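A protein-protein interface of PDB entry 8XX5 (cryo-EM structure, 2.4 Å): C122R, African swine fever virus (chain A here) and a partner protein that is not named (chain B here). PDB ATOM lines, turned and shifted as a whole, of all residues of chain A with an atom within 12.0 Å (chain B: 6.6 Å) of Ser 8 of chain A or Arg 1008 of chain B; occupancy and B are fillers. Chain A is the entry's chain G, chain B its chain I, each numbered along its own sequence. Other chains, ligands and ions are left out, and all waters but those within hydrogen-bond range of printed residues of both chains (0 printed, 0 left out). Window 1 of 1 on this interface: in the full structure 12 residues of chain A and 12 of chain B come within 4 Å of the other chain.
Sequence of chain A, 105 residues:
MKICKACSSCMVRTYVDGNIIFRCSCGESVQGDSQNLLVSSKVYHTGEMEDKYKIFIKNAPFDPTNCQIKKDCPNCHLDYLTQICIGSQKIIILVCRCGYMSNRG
Printed residues of chain B that touch a printed residue of chain A: Arg 1008, Leu 1011, Tyr 1012 and His 1057. Hydrophobic or aromatic side chains of chain B within 4 Å of the printed part of chain A: Leu 1011, Tyr 1012 and His 1057. Along chain A the printed residues that touch a printed residue of chain B span positions 5 to 26. Among the printed residues, 8 pairs touch across the chains.
The backbone NH (N) of Ala 6 of chain A sits close to the side-chain sulfur (SG) of Cys 4 of chain A, 3.6 Å away. The side-chain sulfur of Cys 26 of chain A sits close to the backbone NH of Glu 28 of chain A, at 3.8 Å. The side-chain carboxylate (OD1) of Asp 1004 of chain B is in salt-bridge range of the guanidinium group (NH2) of Arg 1008 of chain B, at 3.6 Å.
NE2 of His 1057 of chain B sits close to O of Lys 5 of chain A, 3.3 Å away. O of Ala 6 of chain A sits at hydrogen-bond distance from NE2 of His 1057 of chain B (2.5 Å). The side-chain hydroxyl of Ser 8 of chain A lies close to the guanidinium group of Arg 1008 of chain B, 3.5 Å away. The side-chain hydroxyl of Tyr 1012 of chain B lies within hydrogen-bond range of the side-chain hydroxyl of Ser 25 of chain A, at 3.2 Å.
Ala 6 of chain A touches Leu 1011 of chain B (O to CD1, 3.7 Å). CD1 of Tyr 1012 of chain B touches SG of Cys 7 of chain A, at 3.5 Å. Ser 8 of chain A touches His 1057 of chain B. Tyr 1012 of chain B touches Cys 26 of chain A (CD1 to CB, 3.6 Å).
Of chain A, only Ser 8 comes within 4 Å of Arg 1008 of chain B. No residue of chain A comes within 4 Å of Asp 1004 of chain B. No residue of chain A comes within 4 Å of Ser 1005 of chain B. No residue of chain A comes within 4 Å of Ala 1006 of chain B. No residue of chain A comes within 4 Å of Val 1007 of chain B. No residue of chain A comes within 4 Å of Ile 1009 of chain B. Leu 1011 of chain B touches just one residue of chain A: Ala 6. His 1057 of chain B touches just these residues of chain A: Lys 5, Ala 6 and Ser 8. Of the printed residues of chain B, Cys 7 of chain A touches Tyr 1012 (3.5 Å). Printed residues of chain B within 4 Å of Ser 25 of chain A: Tyr 1012 (3.2 Å). Of the printed residues of chain A, Tyr 1012 of chain B touches Cys 7 (3.5 Å), Ser 25 (3.2 Å) and Cys 26 (3.6 Å). Printed residues of chain B within 4 Å of Lys 5 of chain A: His 1057 (3.1 Å). Printed residues of chain B within 4 Å of Cys 26 of chain A: Tyr 1012 (3.6 Å). Phe 1060 of chain B touches none of the printed residues of chain A. Cys 4 of chain A touches none of the printed residues of chain B.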
ATOM      1  N   MET A   1      23.451  -8.925  21.332  1.00  0.00           N
ATOM      2  CA  MET A   1      23.221 -10.331  21.638  1.00  0.00           C
ATOM      3  C   MET A   1      24.405 -11.178  21.190  1.00  0.00           C
ATOM      4  O   MET A   1      25.275 -10.708  20.459  1.00  0.00           O
ATOM      5  CB  MET A   1      21.939 -10.824  20.967  1.00  0.00           C
ATOM      6  CG  MET A   1      22.108 -11.170  19.498  1.00  0.00           C
ATOM      7  SD  MET A   1      22.581  -9.747  18.500  1.00  0.00           S
ATOM      8  CE  MET A   1      22.007 -10.261  16.887  1.00  0.00           C
ATOM      9  N   LYS A   2      24.431 -12.432  21.631  1.00  0.00           N
ATOM     10  CA  LYS A   2      25.485 -13.371  21.272  1.00  0.00           C
ATOM     11  C   LYS A   2      24.981 -14.272  20.153  1.00  0.00           C
ATOM     12  O   LYS A   2      23.936 -14.916  20.293  1.00  0.00           O
ATOM     13  CB  LYS A   2      25.911 -14.199  22.482  1.00  0.00           C
ATOM     14  CG  LYS A   2      27.166 -15.026  22.264  1.00  0.00           C
ATOM     15  CD  LYS A   2      28.366 -14.143  21.981  1.00  0.00           C
ATOM     16  CE  LYS A   2      29.220 -13.966  23.225  1.00  0.00           C
ATOM     17  NZ  LYS A   2      30.049 -12.730  23.160  1.00  0.00           N
ATOM     18  N   ILE A   3      25.722 -14.315  19.051  1.00  0.00           N
ATOM     19  CA  ILE A   3      25.378 -15.134  17.896  1.00  0.00           C
ATOM     20  C   ILE A   3      26.202 -16.412  17.949  1.00  0.00           C
ATOM     21  O   ILE A   3      27.435 -16.360  18.045  1.00  0.00           O
ATOM     22  CB  ILE A   3      25.619 -14.376  16.580  1.00  0.00           C
ATOM     23  CG1 ILE A   3      24.607 -13.238  16.428  1.00  0.00           C
ATOM     24  CG2 ILE A   3      25.537 -15.323  15.394  1.00  0.00           C
ATOM     25  CD1 ILE A   3      23.177 -13.709  16.300  1.00  0.00           C
ATOM     26  N   CYS A   4      25.524 -17.556  17.897  1.00  0.00           N
ATOM     27  CA  CYS A   4      26.212 -18.839  17.940  1.00  0.00           C
ATOM     28  C   CYS A   4      27.128 -18.995  16.733  1.00  0.00           C
ATOM     29  O   CYS A   4      26.764 -18.653  15.605  1.00  0.00           O
ATOM     30  CB  CYS A   4      25.195 -19.978  17.997  1.00  0.00           C
ATOM     31  SG  CYS A   4      25.899 -21.634  17.850  1.00  0.00           S
ATOM     32  N   LYS A   5      28.333 -19.511  16.980  1.00  0.00           N
ATOM     33  CA  LYS A   5      29.350 -19.572  15.937  1.00  0.00           C
ATOM     34  C   LYS A   5      29.069 -20.660  14.908  1.00  0.00           C
ATOM     35  O   LYS A   5      29.461 -20.517  13.746  1.00  0.00           O
ATOM     36  CB  LYS A   5      30.728 -19.786  16.564  1.00  0.00           C
ATOM     37  CG  LYS A   5      31.412 -18.500  16.999  1.00  0.00           C
ATOM     38  CD  LYS A   5      32.477 -18.762  18.052  1.00  0.00           C
ATOM     39  CE  LYS A   5      33.869 -18.783  17.444  1.00  0.00           C
ATOM     40  NZ  LYS A   5      34.236 -20.134  16.939  1.00  0.00           N
ATOM     41  N   ALA A   6      28.400 -21.744  15.303  1.00  0.00           N
ATOM     42  CA  ALA A   6      28.092 -22.807  14.353  1.00  0.00           C
ATOM     43  C   ALA A   6      26.880 -22.447  13.503  1.00  0.00           C
ATOM     44  O   ALA A   6      26.985 -22.295  12.282  1.00  0.00           O
ATOM     45  CB  ALA A   6      27.858 -24.125  15.096  1.00  0.00           C
ATOM     46  N   CYS A   7      25.723 -22.302  14.138  1.00  0.00           N
ATOM     47  CA  CYS A   7      24.518 -21.827  13.475  1.00  0.00           C
ATOM     48  C   CYS A   7      24.300 -20.372  13.861  1.00  0.00           C
ATOM     49  O   CYS A   7      24.381 -20.021  15.040  1.00  0.00           O
ATOM     50  CB  CYS A   7      23.305 -22.673  13.862  1.00  0.00           C
ATOM     51  SG  CYS A   7      22.926 -22.679  15.630  1.00  0.00           S
ATOM     52  N   SER A   8      24.026 -19.527  12.871  1.00  0.00           N
ATOM     53  CA  SER A   8      23.901 -18.093  13.117  1.00  0.00           C
ATOM     54  C   SER A   8      22.583 -17.845  13.846  1.00  0.00           C
ATOM     55  O   SER A   8      21.570 -17.450  13.264  1.00  0.00           O
ATOM     56  CB  SER A   8      23.982 -17.319  11.810  1.00  0.00           C
ATOM     57  OG  SER A   8      25.329 -17.111  11.428  1.00  0.00           O
ATOM     58  N   SER A   9      22.602 -18.093  15.153  1.00  0.00           N
ATOM     59  CA  SER A   9      21.413 -17.997  15.985  1.00  0.00           C
ATOM     60  C   SER A   9      21.730 -17.252  17.271  1.00  0.00           C
ATOM     61  O   SER A   9      22.873 -17.240  17.735  1.00  0.00           O
ATOM     62  CB  SER A   9      20.853 -19.385  16.315  1.00  0.00           C
ATOM     63  OG  SER A   9      20.078 -19.350  17.497  1.00  0.00           O
ATOM     64  N   CYS A  10      20.705 -16.624  17.841  1.00  0.00           N
ATOM     65  CA  CYS A  10      20.840 -15.958  19.129  1.00  0.00           C
ATOM     66  C   CYS A  10      20.791 -16.983  20.254  1.00  0.00           C
ATOM     67  O   CYS A  10      20.024 -17.948  20.202  1.00  0.00           O
ATOM     68  CB  CYS A  10      19.736 -14.918  19.321  1.00  0.00           C
ATOM     69  SG  CYS A  10      19.164 -14.128  17.803  1.00  0.00           S
ATOM     70  N   MET A  11      21.612 -16.768  21.276  1.00  0.00           N
ATOM     71  CA  MET A  11      21.731 -17.693  22.392  1.00  0.00           C
ATOM     72  C   MET A  11      21.286 -17.025  23.685  1.00  0.00           C
ATOM     73  O   MET A  11      21.519 -15.830  23.892  1.00  0.00           O
ATOM     74  CB  MET A  11      23.165 -18.204  22.528  1.00  0.00           C
ATOM     75  CG  MET A  11      23.985 -18.090  21.257  1.00  0.00           C
ATOM     76  SD  MET A  11      25.743 -18.300  21.571  1.00  0.00           S
ATOM     77  CE  MET A  11      25.745 -19.948  22.268  1.00  0.00           C
ATOM     78  N   VAL A  12      20.642 -17.807  24.549  1.00  0.00           N
ATOM     79  CA  VAL A  12      20.107 -17.319  25.814  1.00  0.00           C
ATOM     80  C   VAL A  12      21.243 -17.054  26.793  1.00  0.00           C
ATOM     81  O   VAL A  12      22.385 -17.465  26.562  1.00  0.00           O
ATOM     82  CB  VAL A  12      19.091 -18.314  26.399  1.00  0.00           C
ATOM     83  CG1 VAL A  12      18.039 -18.658  25.361  1.00  0.00           C
ATOM     84  CG2 VAL A  12      19.800 -19.570  26.863  1.00  0.00           C
ATOM     85  N   ARG A  23      23.760 -20.267  26.107  1.00  0.00           N
ATOM     86  CA  ARG A  23      23.275 -21.558  25.638  1.00  0.00           C
ATOM     87  C   ARG A  23      22.505 -21.376  24.339  1.00  0.00           C
ATOM     88  O   ARG A  23      21.632 -20.508  24.246  1.00  0.00           O
ATOM     89  CB  ARG A  23      22.380 -22.216  26.686  1.00  0.00           C
ATOM     90  CG  ARG A  23      23.123 -22.972  27.771  1.00  0.00           C
ATOM     91  CD  ARG A  23      23.570 -24.344  27.286  1.00  0.00           C
ATOM     92  NE  ARG A  23      24.930 -24.676  27.698  1.00  0.00           N
ATOM     93  CZ  ARG A  23      25.330 -24.823  28.955  1.00  0.00           C
ATOM     94  NH1 ARG A  23      24.488 -24.710  29.970  1.00  0.00           N
ATOM     95  NH2 ARG A  23      26.606 -25.104  29.200  1.00  0.00           N
ATOM     96  N   CYS A  24      22.826 -22.194  23.345  1.00  0.00           N
ATOM     97  CA  CYS A  24      22.132 -22.188  22.068  1.00  0.00           C
ATOM     98  C   CYS A  24      21.244 -23.421  21.942  1.00  0.00           C
ATOM     99  O   CYS A  24      21.422 -24.419  22.643  1.00  0.00           O
ATOM    100  CB  CYS A  24      23.129 -22.140  20.910  1.00  0.00           C
ATOM    101  SG  CYS A  24      22.364 -22.055  19.280  1.00  0.00           S
ATOM    102  N   SER A  25      20.272 -23.335  21.032  1.00  0.00           N
ATOM    103  CA  SER A  25      19.386 -24.466  20.777  1.00  0.00           C
ATOM    104  C   SER A  25      20.112 -25.650  20.156  1.00  0.00           C
ATOM    105  O   SER A  25      19.575 -26.762  20.176  1.00  0.00           O
ATOM    106  CB  SER A  25      18.232 -24.038  19.871  1.00  0.00           C
ATOM    107  OG  SER A  25      18.715 -23.495  18.655  1.00  0.00           O
ATOM    108  N   CYS A  26      21.307 -25.440  19.611  1.00  0.00           N
ATOM    109  CA  CYS A  26      22.130 -26.513  19.073  1.00  0.00           C
ATOM    110  C   CYS A  26      23.107 -27.071  20.102  1.00  0.00           C
ATOM    111  O   CYS A  26      23.932 -27.921  19.758  1.00  0.00           O
ATOM    112  CB  CYS A  26      22.885 -26.024  17.836  1.00  0.00           C
ATOM    113  SG  CYS A  26      24.382 -25.080  18.188  1.00  0.00           S
ATOM    114  N   GLY A  27      23.034 -26.609  21.349  1.00  0.00           N
ATOM    115  CA  GLY A  27      23.846 -27.137  22.422  1.00  0.00           C
ATOM    116  C   GLY A  27      25.177 -26.449  22.631  1.00  0.00           C
ATOM    117  O   GLY A  27      25.870 -26.765  23.606  1.00  0.00           O
ATOM    118  N   GLU A  28      25.558 -25.523  21.757  1.00  0.00           N
ATOM    119  CA  GLU A  28      26.841 -24.852  21.891  1.00  0.00           C
ATOM    120  C   GLU A  28      26.835 -23.891  23.076  1.00  0.00           C
ATOM    121  O   GLU A  28      25.834 -23.231  23.369  1.00  0.00           O
ATOM    122  CB  GLU A  28      27.182 -24.103  20.602  1.00  0.00           C
ATOM    123  CG  GLU A  28      28.369 -23.164  20.709  1.00  0.00           C
ATOM    124  CD  GLU A  28      29.576 -23.661  19.943  1.00  0.00           C
ATOM    125  OE1 GLU A  28      29.625 -24.867  19.627  1.00  0.00           O
ATOM    126  OE2 GLU A  28      30.479 -22.846  19.659  1.00  0.00           O
ATOM    127  N   VAL A  30      29.467 -20.850  24.966  1.00  0.00           N
ATOM    128  CA  VAL A  30      30.579 -19.959  24.651  1.00  0.00           C
ATOM    129  C   VAL A  30      31.208 -19.332  25.887  1.00  0.00           C
ATOM    130  O   VAL A  30      32.270 -18.701  25.768  1.00  0.00           O
ATOM    131  CB  VAL A  30      30.137 -18.854  23.660  1.00  0.00           C
ATOM    132  CG1 VAL A  30      31.334 -18.137  23.040  1.00  0.00           C
ATOM    133  CG2 VAL A  30      29.257 -19.438  22.572  1.00  0.00           C
ATOM    134  N   MET B1001      21.032 -17.392  -0.302  1.00  0.00           N
ATOM    135  CA  MET B1001      20.392 -17.619   0.989  1.00  0.00           C
ATOM    136  C   MET B1001      19.951 -19.068   1.138  1.00  0.00           C
ATOM    137  O   MET B1001      20.041 -19.638   2.227  1.00  0.00           O
ATOM    138  CB  MET B1001      19.206 -16.672   1.161  1.00  0.00           C
ATOM    139  CG  MET B1001      19.424 -15.590   2.203  1.00  0.00           C
ATOM    140  SD  MET B1001      20.962 -14.682   1.961  1.00  0.00           S
ATOM    141  CE  MET B1001      20.704 -14.006   0.321  1.00  0.00           C
ATOM    142  N   VAL B1003      21.302 -21.863  -0.266  1.00  0.00           N
ATOM    143  CA  VAL B1003      22.442 -22.739  -0.008  1.00  0.00           C
ATOM    144  C   VAL B1003      23.035 -22.458   1.368  1.00  0.00           C
ATOM    145  O   VAL B1003      23.487 -23.378   2.065  1.00  0.00           O
ATOM    146  CB  VAL B1003      23.496 -22.609  -1.121  1.00  0.00           C
ATOM    147  CG1 VAL B1003      24.533 -23.701  -0.977  1.00  0.00           C
ATOM    148  CG2 VAL B1003      22.838 -22.715  -2.477  1.00  0.00           C
ATOM    149  N   ASP B1004      23.045 -21.188   1.784  1.00  0.00           N
ATOM    150  CA  ASP B1004      23.483 -20.866   3.136  1.00  0.00           C
ATOM    151  C   ASP B1004      22.587 -21.527   4.172  1.00  0.00           C
ATOM    152  O   ASP B1004      23.068 -22.004   5.202  1.00  0.00           O
ATOM    153  CB  ASP B1004      23.503 -19.352   3.332  1.00  0.00           C
ATOM    154  CG  ASP B1004      24.207 -18.939   4.605  1.00  0.00           C
ATOM    155  OD1 ASP B1004      25.241 -19.550   4.941  1.00  0.00           O
ATOM    156  OD2 ASP B1004      23.725 -18.001   5.273  1.00  0.00           O
ATOM    157  N   SER B1005      21.280 -21.567   3.915  1.00  0.00           N
ATOM    158  CA  SER B1005      20.356 -22.233   4.825  1.00  0.00           C
ATOM    159  C   SER B1005      20.611 -23.734   4.874  1.00  0.00           C
ATOM    160  O   SER B1005      20.492 -24.355   5.937  1.00  0.00           O
ATOM    161  CB  SER B1005      18.915 -21.944   4.406  1.00  0.00           C
ATOM    162  OG  SER B1005      18.386 -23.006   3.636  1.00  0.00           O
ATOM    163  N   ALA B1006      20.936 -24.337   3.730  1.00  0.00           N
ATOM    164  CA  ALA B1006      21.273 -25.760   3.720  1.00  0.00           C
ATOM    165  C   ALA B1006      22.523 -26.034   4.551  1.00  0.00           C
ATOM    166  O   ALA B1006      22.555 -26.964   5.371  1.00  0.00           O
ATOM    167  CB  ALA B1006      21.462 -26.241   2.281  1.00  0.00           C
ATOM    168  N   VAL B1007      23.563 -25.219   4.364  1.00  0.00           N
ATOM    169  CA  VAL B1007      24.770 -25.370   5.172  1.00  0.00           C
ATOM    170  C   VAL B1007      24.450 -25.150   6.646  1.00  0.00           C
ATOM    171  O   VAL B1007      24.984 -25.838   7.525  1.00  0.00           O
ATOM    172  CB  VAL B1007      25.870 -24.412   4.681  1.00  0.00           C
ATOM    173  CG1 VAL B1007      27.086 -24.497   5.584  1.00  0.00           C
ATOM    174  CG2 VAL B1007      26.254 -24.731   3.249  1.00  0.00           C
ATOM    175  N   ARG B1008      23.572 -24.189   6.936  1.00  0.00           N
ATOM    176  CA  ARG B1008      23.215 -23.884   8.315  1.00  0.00           C
ATOM    177  C   ARG B1008      22.492 -25.046   8.976  1.00  0.00           C
ATOM    178  O   ARG B1008      22.757 -25.359  10.138  1.00  0.00           O
ATOM    179  CB  ARG B1008      22.352 -22.625   8.366  1.00  0.00           C
ATOM    180  CG  ARG B1008      21.784 -22.321   9.742  1.00  0.00           C
ATOM    181  CD  ARG B1008      21.558 -20.832   9.941  1.00  0.00           C
ATOM    182  NE  ARG B1008      21.626 -20.086   8.691  1.00  0.00           N
ATOM    183  CZ  ARG B1008      22.633 -19.300   8.341  1.00  0.00           C
ATOM    184  NH1 ARG B1008      23.693 -19.148   9.114  1.00  0.00           N
ATOM    185  NH2 ARG B1008      22.574 -18.650   7.182  1.00  0.00           N
ATOM    186  N   ILE B1009      21.561 -25.686   8.266  1.00  0.00           N
ATOM    187  CA  ILE B1009      20.857 -26.817   8.863  1.00  0.00           C
ATOM    188  C   ILE B1009      21.808 -27.991   9.052  1.00  0.00           C
ATOM    189  O   ILE B1009      21.738 -28.705  10.063  1.00  0.00           O
ATOM    190  CB  ILE B1009      19.607 -27.197   8.044  1.00  0.00           C
ATOM    191  CG1 ILE B1009      18.755 -28.206   8.817  1.00  0.00           C
ATOM    192  CG2 ILE B1009      19.966 -27.773   6.692  1.00  0.00           C
ATOM    193  CD1 ILE B1009      17.676 -27.579   9.663  1.00  0.00           C
ATOM    194  N   PHE B1010      22.739 -28.190   8.111  1.00  0.00           N
ATOM    195  CA  PHE B1010      23.756 -29.220   8.307  1.00  0.00           C
ATOM    196  C   PHE B1010      24.565 -28.962   9.573  1.00  0.00           C
ATOM    197  O   PHE B1010      24.737 -29.856  10.410  1.00  0.00           O
ATOM    198  CB  PHE B1010      24.676 -29.296   7.089  1.00  0.00           C
ATOM    199  CG  PHE B1010      25.664 -30.425   7.153  1.00  0.00           C
ATOM    200  CD1 PHE B1010      25.299 -31.702   6.768  1.00  0.00           C
ATOM    201  CD2 PHE B1010      26.954 -30.210   7.601  1.00  0.00           C
ATOM    202  CE1 PHE B1010      26.202 -32.744   6.829  1.00  0.00           C
ATOM    203  CE2 PHE B1010      27.863 -31.248   7.664  1.00  0.00           C
ATOM    204  CZ  PHE B1010      27.486 -32.516   7.276  1.00  0.00           C
ATOM    205  N   LEU B1011      25.061 -27.732   9.736  1.00  0.00           N
ATOM    206  CA  LEU B1011      25.886 -27.409  10.897  1.00  0.00           C
ATOM    207  C   LEU B1011      25.082 -27.472  12.191  1.00  0.00           C
ATOM    208  O   LEU B1011      25.600 -27.901  13.229  1.00  0.00           O
ATOM    209  CB  LEU B1011      26.514 -26.027  10.723  1.00  0.00           C
ATOM    210  CG  LEU B1011      27.538 -25.890   9.596  1.00  0.00           C
ATOM    211  CD1 LEU B1011      28.134 -24.494   9.579  1.00  0.00           C
ATOM    212  CD2 LEU B1011      28.627 -26.939   9.731  1.00  0.00           C
ATOM    213  N   TYR B1012      23.821 -27.043  12.149  1.00  0.00           N
ATOM    214  CA  TYR B1012      22.969 -27.085  13.331  1.00  0.00           C
ATOM    215  C   TYR B1012      22.745 -28.519  13.789  1.00  0.00           C
ATOM    216  O   TYR B1012      22.872 -28.832  14.979  1.00  0.00           O
ATOM    217  CB  TYR B1012      21.637 -26.398  13.024  1.00  0.00           C
ATOM    218  CG  TYR B1012      20.657 -26.383  14.174  1.00  0.00           C
ATOM    219  CD1 TYR B1012      20.673 -25.360  15.109  1.00  0.00           C
ATOM    220  CD2 TYR B1012      19.706 -27.383  14.314  1.00  0.00           C
ATOM    221  CE1 TYR B1012      19.778 -25.338  16.157  1.00  0.00           C
ATOM    222  CE2 TYR B1012      18.808 -27.371  15.360  1.00  0.00           C
ATOM    223  CZ  TYR B1012      18.848 -26.347  16.278  1.00  0.00           C
ATOM    224  OH  TYR B1012      17.953 -26.328  17.322  1.00  0.00           O
ATOM    225  N   ASN B1013      22.419 -29.410  12.852  1.00  0.00           N
ATOM    226  CA  ASN B1013      22.209 -30.802  13.225  1.00  0.00           C
ATOM    227  C   ASN B1013      23.510 -31.468  13.653  1.00  0.00           C
ATOM    228  O   ASN B1013      23.501 -32.325  14.545  1.00  0.00           O
ATOM    229  CB  ASN B1013      21.548 -31.549  12.069  1.00  0.00           C
ATOM    230  CG  ASN B1013      20.078 -31.205  11.929  1.00  0.00           C
ATOM    231  OD1 ASN B1013      19.414 -30.873  12.909  1.00  0.00           O
ATOM    232  ND2 ASN B1013      19.566 -31.266  10.708  1.00  0.00           N
ATOM    233  N   TYR B1056      33.243 -20.532   7.957  1.00  0.00           N
ATOM    234  CA  TYR B1056      32.278 -20.511   6.865  1.00  0.00           C
ATOM    235  C   TYR B1056      31.481 -19.213   6.832  1.00  0.00           C
ATOM    236  O   TYR B1056      31.241 -18.660   5.756  1.00  0.00           O
ATOM    237  CB  TYR B1056      31.322 -21.696   6.971  1.00  0.00           C
ATOM    238  CG  TYR B1056      30.111 -21.535   6.082  1.00  0.00           C
ATOM    239  CD1 TYR B1056      30.222 -21.638   4.705  1.00  0.00           C
ATOM    240  CD2 TYR B1056      28.864 -21.247   6.619  1.00  0.00           C
ATOM    241  CE1 TYR B1056      29.126 -21.479   3.887  1.00  0.00           C
ATOM    242  CE2 TYR B1056      27.763 -21.085   5.810  1.00  0.00           C
ATOM    243  CZ  TYR B1056      27.897 -21.203   4.444  1.00  0.00           C
ATOM    244  OH  TYR B1056      26.801 -21.042   3.631  1.00  0.00           O
ATOM    245  N   HIS B1057      31.044 -18.723   7.992  1.00  0.00           N
ATOM    246  CA  HIS B1057      30.101 -17.609   8.010  1.00  0.00           C
ATOM    247  C   HIS B1057      30.748 -16.317   7.522  1.00  0.00           C
ATOM    248  O   HIS B1057      30.182 -15.607   6.682  1.00  0.00           O
ATOM    249  CB  HIS B1057      29.529 -17.439   9.416  1.00  0.00           C
ATOM    250  CG  HIS B1057      28.721 -18.612   9.878  1.00  0.00           C
ATOM    251  ND1 HIS B1057      27.544 -18.990   9.268  1.00  0.00           N
ATOM    252  CD2 HIS B1057      28.924 -19.494  10.883  1.00  0.00           C
ATOM    253  CE1 HIS B1057      27.056 -20.053   9.881  1.00  0.00           C
ATOM    254  NE2 HIS B1057      27.873 -20.379  10.865  1.00  0.00           N
ATOM    255  N   PHE B1060      31.551 -16.604   3.801  1.00  0.00           N
ATOM    256  CA  PHE B1060      30.335 -16.538   3.003  1.00  0.00           C
ATOM    257  C   PHE B1060      29.801 -15.119   2.926  1.00  0.00           C
ATOM    258  O   PHE B1060      29.369 -14.677   1.860  1.00  0.00           O
ATOM    259  CB  PHE B1060      29.263 -17.467   3.566  1.00  0.00           C
ATOM    260  CG  PHE B1060      27.935 -17.316   2.884  1.00  0.00           C
ATOM    261  CD1 PHE B1060      27.744 -17.795   1.600  1.00  0.00           C
ATOM    262  CD2 PHE B1060      26.886 -16.666   3.512  1.00  0.00           C
ATOM    263  CE1 PHE B1060      26.530 -17.649   0.964  1.00  0.00           C
ATOM    264  CE2 PHE B1060      25.670 -16.513   2.877  1.00  0.00           C
ATOM    265  CZ  PHE B1060      25.491 -17.006   1.603  1.00  0.00           C
ATOM    266  N   LEU B1079      29.628 -27.421   1.973  1.00  0.00           N
ATOM    267  CA  LEU B1079      28.731 -28.496   2.384  1.00  0.00           C
ATOM    268  C   LEU B1079      29.307 -29.856   2.005  1.00  0.00           C
ATOM    269  O   LEU B1079      29.305 -30.792   2.817  1.00  0.00           O
ATOM    270  CB  LEU B1079      27.354 -28.292   1.755  1.00  0.00           C
ATOM    271  CG  LEU B1079      26.268 -29.319   2.069  1.00  0.00           C
ATOM    272  CD1 LEU B1079      25.739 -29.126   3.478  1.00  0.00           C
ATOM    273  CD2 LEU B1079      25.142 -29.214   1.054  1.00  0.00           C
